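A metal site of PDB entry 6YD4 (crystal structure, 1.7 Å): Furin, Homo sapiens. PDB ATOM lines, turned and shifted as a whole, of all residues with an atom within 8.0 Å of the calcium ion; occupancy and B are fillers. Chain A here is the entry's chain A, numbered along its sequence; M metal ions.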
ATOM      1  N   PRO A   6      26.897  -6.672  -4.834  1.00  0.00           N
ATOM      2  CA  PRO A   6      25.811  -7.612  -5.116  1.00  0.00           C
ATOM      3  C   PRO A   6      24.639  -7.482  -4.160  1.00  0.00           C
ATOM      4  O   PRO A   6      24.814  -7.206  -2.972  1.00  0.00           O
ATOM      5  CB  PRO A   6      26.484  -8.987  -4.967  1.00  0.00           C
ATOM      6  CG  PRO A   6      27.893  -8.736  -5.379  1.00  0.00           C
ATOM      7  CD  PRO A   6      28.212  -7.341  -4.859  1.00  0.00           C
ATOM      8  N   THR A   7      23.447  -7.754  -4.697  1.00  0.00           N
ATOM      9  CA  THR A   7      22.206  -7.772  -3.940  1.00  0.00           C
ATOM     10  C   THR A   7      21.755  -9.183  -3.595  1.00  0.00           C
ATOM     11  O   THR A   7      20.682  -9.346  -3.020  1.00  0.00           O
ATOM     12  CB  THR A   7      21.129  -7.063  -4.760  1.00  0.00           C
ATOM     13  OG1 THR A   7      21.026  -7.678  -6.044  1.00  0.00           O
ATOM     14  CG2 THR A   7      21.507  -5.600  -4.952  1.00  0.00           C
ATOM     15  N   ASP A   8      22.554 -10.196  -3.921  1.00  0.00           N
ATOM     16  CA  ASP A   8      22.131 -11.567  -3.698  1.00  0.00           C
ATOM     17  C   ASP A   8      21.774 -11.795  -2.241  1.00  0.00           C
ATOM     18  O   ASP A   8      22.385 -11.207  -1.337  1.00  0.00           O
ATOM     19  CB  ASP A   8      23.234 -12.526  -4.138  1.00  0.00           C
ATOM     20  CG  ASP A   8      23.656 -12.305  -5.576  1.00  0.00           C
ATOM     21  OD1 ASP A   8      24.173 -11.212  -5.884  1.00  0.00           O
ATOM     22  OD2 ASP A   8      23.454 -13.213  -6.407  1.00  0.00           O
ATOM     23  N   PRO A   9      20.802 -12.687  -1.978  1.00  0.00           N
ATOM     24  CA  PRO A   9      20.264 -12.815  -0.618  1.00  0.00           C
ATOM     25  C   PRO A   9      21.271 -13.256   0.416  1.00  0.00           C
ATOM     26  O   PRO A   9      21.137 -12.864   1.581  1.00  0.00           O
ATOM     27  CB  PRO A   9      19.131 -13.846  -0.771  1.00  0.00           C
ATOM     28  CG  PRO A   9      19.368 -14.520  -2.084  1.00  0.00           C
ATOM     29  CD  PRO A   9      20.053 -13.494  -2.959  1.00  0.00           C
ATOM     30  N   LYS A  10      22.246 -14.079   0.050  1.00  0.00           N
ATOM     31  CA  LYS A  10      23.237 -14.577   1.000  1.00  0.00           C
ATOM     32  C   LYS A  10      24.556 -13.817   0.907  1.00  0.00           C
ATOM     33  O   LYS A  10      25.497 -14.144   1.637  1.00  0.00           O
ATOM     34  CB  LYS A  10      23.491 -16.070   0.769  1.00  0.00           C
ATOM     35  CG  LYS A  10      22.256 -16.943   0.825  1.00  0.00           C
ATOM     36  CD  LYS A  10      21.620 -16.911   2.199  1.00  0.00           C
ATOM     37  CE  LYS A  10      20.311 -17.685   2.240  1.00  0.00           C
ATOM     38  NZ  LYS A  10      19.625 -17.517   3.561  1.00  0.00           N
ATOM     39  N   PHE A  11      24.662 -12.807   0.041  1.00  0.00           N
ATOM     40  CA  PHE A  11      25.905 -12.056  -0.027  1.00  0.00           C
ATOM     41  C   PHE A  11      26.274 -11.442   1.320  1.00  0.00           C
ATOM     42  O   PHE A  11      27.469 -11.429   1.665  1.00  0.00           O
ATOM     43  CB  PHE A  11      25.840 -10.966  -1.103  1.00  0.00           C
ATOM     44  CG  PHE A  11      27.043 -10.070  -1.114  1.00  0.00           C
ATOM     45  CD1 PHE A  11      28.273 -10.544  -1.539  1.00  0.00           C
ATOM     46  CD2 PHE A  11      26.954  -8.750  -0.705  1.00  0.00           C
ATOM     47  CE1 PHE A  11      29.377  -9.728  -1.535  1.00  0.00           C
ATOM     48  CE2 PHE A  11      28.065  -7.925  -0.713  1.00  0.00           C
ATOM     49  CZ  PHE A  11      29.276  -8.429  -1.132  1.00  0.00           C
ATOM     50  N   GLN A  14      28.630 -13.562   3.291  1.00  0.00           N
ATOM     51  CA  GLN A  14      29.946 -13.877   2.723  1.00  0.00           C
ATOM     52  C   GLN A  14      30.994 -12.948   3.341  1.00  0.00           C
ATOM     53  O   GLN A  14      31.571 -12.053   2.712  1.00  0.00           O
ATOM     54  CB  GLN A  14      29.882 -13.801   1.196  1.00  0.00           C
ATOM     55  CG  GLN A  14      28.883 -14.796   0.616  1.00  0.00           C
ATOM     56  CD  GLN A  14      28.915 -14.917  -0.881  1.00  0.00           C
ATOM     57  OE1 GLN A  14      28.266 -14.153  -1.593  1.00  0.00           O
ATOM     58  NE2 GLN A  14      29.701 -15.875  -1.384  1.00  0.00           N
ATOM     59  N   HIS A  53      22.565 -25.594 -12.303  1.00  0.00           N
ATOM     60  CA  HIS A  53      22.291 -24.953 -11.021  1.00  0.00           C
ATOM     61  C   HIS A  53      21.868 -23.503 -11.255  1.00  0.00           C
ATOM     62  O   HIS A  53      22.512 -22.813 -12.062  1.00  0.00           O
ATOM     63  CB  HIS A  53      23.522 -25.020 -10.104  1.00  0.00           C
ATOM     64  CG  HIS A  53      23.223 -24.658  -8.680  1.00  0.00           C
ATOM     65  ND1 HIS A  53      22.876 -23.383  -8.289  1.00  0.00           N
ATOM     66  CD2 HIS A  53      23.186 -25.424  -7.562  1.00  0.00           C
ATOM     67  CE1 HIS A  53      22.643 -23.373  -6.989  1.00  0.00           C
ATOM     68  NE2 HIS A  53      22.838 -24.594  -6.518  1.00  0.00           N
ATOM     69  N   PRO A  54      20.813 -23.026 -10.597  1.00  0.00           N
ATOM     70  CA  PRO A  54      20.357 -21.647 -10.839  1.00  0.00           C
ATOM     71  C   PRO A  54      21.425 -20.590 -10.604  1.00  0.00           C
ATOM     72  O   PRO A  54      21.313 -19.487 -11.172  1.00  0.00           O
ATOM     73  CB  PRO A  54      19.169 -21.475  -9.863  1.00  0.00           C
ATOM     74  CG  PRO A  54      19.192 -22.690  -8.952  1.00  0.00           C
ATOM     75  CD  PRO A  54      19.919 -23.782  -9.707  1.00  0.00           C
ATOM     76  N   ASP A  55      22.460 -20.870  -9.804  1.00  0.00           N
ATOM     77  CA  ASP A  55      23.527 -19.908  -9.622  1.00  0.00           C
ATOM     78  C   ASP A  55      24.794 -20.242 -10.394  1.00  0.00           C
ATOM     79  O   ASP A  55      25.805 -19.533 -10.230  1.00  0.00           O
ATOM     80  CB  ASP A  55      23.870 -19.753  -8.127  1.00  0.00           C
ATOM     81  CG  ASP A  55      23.901 -18.299  -7.681  1.00  0.00           C
ATOM     82  OD1 ASP A  55      23.308 -17.431  -8.362  1.00  0.00           O
ATOM     83  OD2 ASP A  55      24.526 -18.010  -6.640  1.00  0.00           O
ATOM     84  N   LEU A  56      24.797 -21.297 -11.209  1.00  0.00           N
ATOM     85  CA  LEU A  56      25.944 -21.581 -12.085  1.00  0.00           C
ATOM     86  C   LEU A  56      25.603 -21.513 -13.569  1.00  0.00           C
ATOM     87  O   LEU A  56      26.500 -21.232 -14.377  1.00  0.00           O
ATOM     88  CB  LEU A  56      26.534 -22.962 -11.777  1.00  0.00           C
ATOM     89  CG  LEU A  56      27.027 -23.173 -10.349  1.00  0.00           C
ATOM     90  CD1 LEU A  56      27.448 -24.625 -10.126  1.00  0.00           C
ATOM     91  CD2 LEU A  56      28.183 -22.238 -10.018  1.00  0.00           C
ATOM     92  N   GLY A  93      30.791 -22.869  -7.125  1.00  0.00           N
ATOM     93  CA  GLY A  93      30.084 -21.650  -6.753  1.00  0.00           C
ATOM     94  C   GLY A  93      30.949 -20.653  -6.025  1.00  0.00           C
ATOM     95  O   GLY A  93      30.683 -19.444  -6.062  1.00  0.00           O
ATOM     96  N   ALA A  96      32.587 -18.839  -9.041  1.00  0.00           N
ATOM     97  CA  ALA A  96      31.869 -18.138 -10.112  1.00  0.00           C
ATOM     98  C   ALA A  96      30.363 -18.226 -10.003  1.00  0.00           C
ATOM     99  O   ALA A  96      29.680 -18.183 -11.032  1.00  0.00           O
ATOM    100  CB  ALA A  96      32.288 -18.675 -11.492  1.00  0.00           C
ATOM    101  N   ALA A  97      29.816 -18.338  -8.797  1.00  0.00           N
ATOM    102  CA  ALA A  97      28.368 -18.192  -8.658  1.00  0.00           C
ATOM    103  C   ALA A  97      27.921 -16.841  -9.226  1.00  0.00           C
ATOM    104  O   ALA A  97      28.565 -15.812  -9.021  1.00  0.00           O
ATOM    105  CB  ALA A  97      27.929 -18.321  -7.205  1.00  0.00           C
ATOM    106  N   VAL A  98      26.779 -16.856  -9.938  1.00  0.00           N
ATOM    107  CA  VAL A  98      26.271 -15.656 -10.613  1.00  0.00           C
ATOM    108  C   VAL A  98      25.849 -14.618  -9.585  1.00  0.00           C
ATOM    109  O   VAL A  98      25.360 -14.930  -8.504  1.00  0.00           O
ATOM    110  CB  VAL A  98      25.081 -16.050 -11.518  1.00  0.00           C
ATOM    111  CG1 VAL A  98      24.395 -14.819 -12.162  1.00  0.00           C
ATOM    112  CG2 VAL A  98      25.526 -17.052 -12.585  1.00  0.00           C
ATOM    113  N   ALA A  99      26.053 -13.341  -9.942  1.00  0.00           N
ATOM    114  CA  ALA A  99      25.707 -12.244  -9.055  1.00  0.00           C
ATOM    115  C   ALA A  99      24.416 -11.564  -9.495  1.00  0.00           C
ATOM    116  O   ALA A  99      24.022 -11.631 -10.661  1.00  0.00           O
ATOM    117  CB  ALA A  99      26.823 -11.202  -8.991  1.00  0.00           C
ATOM    118  N   ASN A 100      23.766 -10.906  -8.532  1.00  0.00           N
ATOM    119  CA  ASN A 100      22.609 -10.045  -8.757  1.00  0.00           C
ATOM    120  C   ASN A 100      21.480 -10.785  -9.489  1.00  0.00           C
ATOM    121  O   ASN A 100      20.835 -10.238 -10.387  1.00  0.00           O
ATOM    122  CB  ASN A 100      23.009  -8.793  -9.527  1.00  0.00           C
ATOM    123  CG  ASN A 100      23.973  -7.931  -8.755  1.00  0.00           C
ATOM    124  OD1 ASN A 100      23.711  -7.514  -7.619  1.00  0.00           O
ATOM    125  ND2 ASN A 100      25.121  -7.660  -9.364  1.00  0.00           N
ATOM    126  N   ASN A 101      21.224 -12.017  -9.085  1.00  0.00           N
ATOM    127  CA  ASN A 101      20.179 -12.835  -9.693  1.00  0.00           C
ATOM    128  C   ASN A 101      19.214 -13.367  -8.646  1.00  0.00           C
ATOM    129  O   ASN A 101      18.444 -14.275  -8.930  1.00  0.00           O
ATOM    130  CB  ASN A 101      20.784 -13.983 -10.502  1.00  0.00           C
ATOM    131  CG  ASN A 101      21.473 -15.013  -9.631  1.00  0.00           C
ATOM    132  OD1 ASN A 101      21.825 -14.748  -8.474  1.00  0.00           O
ATOM    133  ND2 ASN A 101      21.650 -16.213 -10.170  1.00  0.00           N
ATOM    134  N   GLY A 102      19.232 -12.800  -7.433  1.00  0.00           N
ATOM    135  CA  GLY A 102      18.315 -13.232  -6.403  1.00  0.00           C
ATOM    136  C   GLY A 102      18.511 -14.629  -5.866  1.00  0.00           C
ATOM    137  O   GLY A 102      17.647 -15.108  -5.149  1.00  0.00           O
ATOM    138  N   VAL A 103      19.644 -15.283  -6.155  1.00  0.00           N
ATOM    139  CA  VAL A 103      19.881 -16.659  -5.729  1.00  0.00           C
ATOM    140  C   VAL A 103      21.182 -16.714  -4.928  1.00  0.00           C
ATOM    141  O   VAL A 103      22.200 -16.179  -5.373  1.00  0.00           O
ATOM    142  CB  VAL A 103      19.972 -17.608  -6.949  1.00  0.00           C
ATOM    143  CG1 VAL A 103      20.353 -19.010  -6.507  1.00  0.00           C
ATOM    144  CG2 VAL A 103      18.636 -17.620  -7.716  1.00  0.00           C
ATOM    145  N   CYS A 104      21.133 -17.367  -3.767  1.00  0.00           N
ATOM    146  CA  CYS A 104      22.323 -17.703  -2.951  1.00  0.00           C
ATOM    147  C   CYS A 104      23.265 -16.499  -2.848  1.00  0.00           C
ATOM    148  O   CYS A 104      22.783 -15.401  -2.518  1.00  0.00           O
ATOM    149  CB  CYS A 104      22.941 -18.981  -3.526  1.00  0.00           C
ATOM    150  SG  CYS A 104      24.049 -19.882  -2.377  1.00  0.00           S
ATOM    151  N   GLY A 105      24.583 -16.680  -3.030  1.00  0.00           N
ATOM    152  CA  GLY A 105      25.525 -15.575  -2.919  1.00  0.00           C
ATOM    153  C   GLY A 105      26.202 -15.292  -4.248  1.00  0.00           C
ATOM    154  O   GLY A 105      25.566 -15.381  -5.294  1.00  0.00           O
ATOM    155  N   VAL A 106      27.498 -14.995  -4.233  1.00  0.00           N
ATOM    156  CA  VAL A 106      28.215 -14.682  -5.459  1.00  0.00           C
ATOM    157  C   VAL A 106      29.569 -15.377  -5.439  1.00  0.00           C
ATOM    158  O   VAL A 106      30.157 -15.588  -4.367  1.00  0.00           O
ATOM    159  CB  VAL A 106      28.426 -13.162  -5.676  1.00  0.00           C
ATOM    160  CG1 VAL A 106      27.100 -12.399  -5.606  1.00  0.00           C
ATOM    161  CG2 VAL A 106      29.433 -12.621  -4.669  1.00  0.00           C
ATOM    162  N   GLY A 107      30.077 -15.685  -6.621  1.00  0.00           N
ATOM    163  CA  GLY A 107      31.468 -16.111  -6.734  1.00  0.00           C
ATOM    164  C   GLY A 107      32.425 -14.949  -6.549  1.00  0.00           C
ATOM    165  O   GLY A 107      32.068 -13.771  -6.689  1.00  0.00           O
ATOM    166  N   TYR A 110      32.488 -13.469 -10.299  1.00  0.00           N
ATOM    167  CA  TYR A 110      31.102 -13.814 -10.619  1.00  0.00           C
ATOM    168  C   TYR A 110      30.738 -13.574 -12.074  1.00  0.00           C
ATOM    169  O   TYR A 110      29.606 -13.911 -12.453  1.00  0.00           O
ATOM    170  CB  TYR A 110      30.152 -13.081  -9.688  1.00  0.00           C
ATOM    171  CG  TYR A 110      30.264 -11.568  -9.620  1.00  0.00           C
ATOM    172  CD1 TYR A 110      29.882 -10.753 -10.693  1.00  0.00           C
ATOM    173  CD2 TYR A 110      30.653 -10.949  -8.441  1.00  0.00           C
ATOM    174  CE1 TYR A 110      29.937  -9.379 -10.602  1.00  0.00           C
ATOM    175  CE2 TYR A 110      30.681  -9.563  -8.325  1.00  0.00           C
ATOM    176  CZ  TYR A 110      30.318  -8.788  -9.409  1.00  0.00           C
ATOM    177  OH  TYR A 110      30.362  -7.404  -9.316  1.00  0.00           O
ATOM    178  N   THR A 247      27.043 -22.697  -3.857  1.00  0.00           N
ATOM    179  CA  THR A 247      26.066 -23.521  -4.538  1.00  0.00           C
ATOM    180  C   THR A 247      26.174 -24.976  -4.091  1.00  0.00           C
ATOM    181  O   THR A 247      27.273 -25.540  -4.024  1.00  0.00           O
ATOM    182  CB  THR A 247      26.290 -23.449  -6.048  1.00  0.00           C
ATOM    183  OG1 THR A 247      27.690 -23.669  -6.334  1.00  0.00           O
ATOM    184  CG2 THR A 247      25.920 -22.095  -6.589  1.00  0.00           C
ATOM    185  N   CYS A 253      21.402 -23.937  -1.902  1.00  0.00           N
ATOM    186  CA  CYS A 253      22.407 -23.008  -1.399  1.00  0.00           C
ATOM    187  C   CYS A 253      22.846 -23.495  -0.029  1.00  0.00           C
ATOM    188  O   CYS A 253      22.003 -23.865   0.797  1.00  0.00           O
ATOM    189  CB  CYS A 253      21.793 -21.605  -1.347  1.00  0.00           C
ATOM    190  SG  CYS A 253      22.862 -20.309  -0.786  1.00  0.00           S
HETATM  191 CA    CA M   1      23.782 -15.534  -6.925  1.00  0.00          CA
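Within 4 Å of the calcium ion: Asp 8, Asp 55, Val 98, Asn 101, Val 103 and Gly 105.
The nearest printed residue that does not touch the calcium ion is Cys 104 (4.2 Å).
O of Val 103 is bound to the calcium ion, at 2.3 Å.
O of Val 98 binds the calcium ion, 2.3 Å away.
The side-chain carboxylate (OD2) of Asp 8 is bound to the calcium ion (2.4 Å).
The calcium ion is bound by the backbone carbonyl oxygen (O) of Gly 105 (2.4 Å).
OD1 of Asp 55 binds the calcium ion, 2.4 Å away.
The calcium ion is bound by OD2 of Asp 55, 2.6 Å away.
OD1 of Asn 101 binds the calcium ion (2.6 Å).
SG of Cys 104 forms a disulfide with SG of Cys 253 (2.0 Å).
The side-chain amide nitrogen (ND2) of Asn 101 lies within hydrogen-bond range of the backbone carbonyl oxygen (O) of Pro 54 (3.4 Å).
A ring nitrogen (ND1) of His 53 is in hydrogen-bond range of the backbone NH (N) of Asp 55 (3.0 Å).
OD1 of Asp 8 is in hydrogen-bond range of N of Asn 100, at 2.7 Å.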
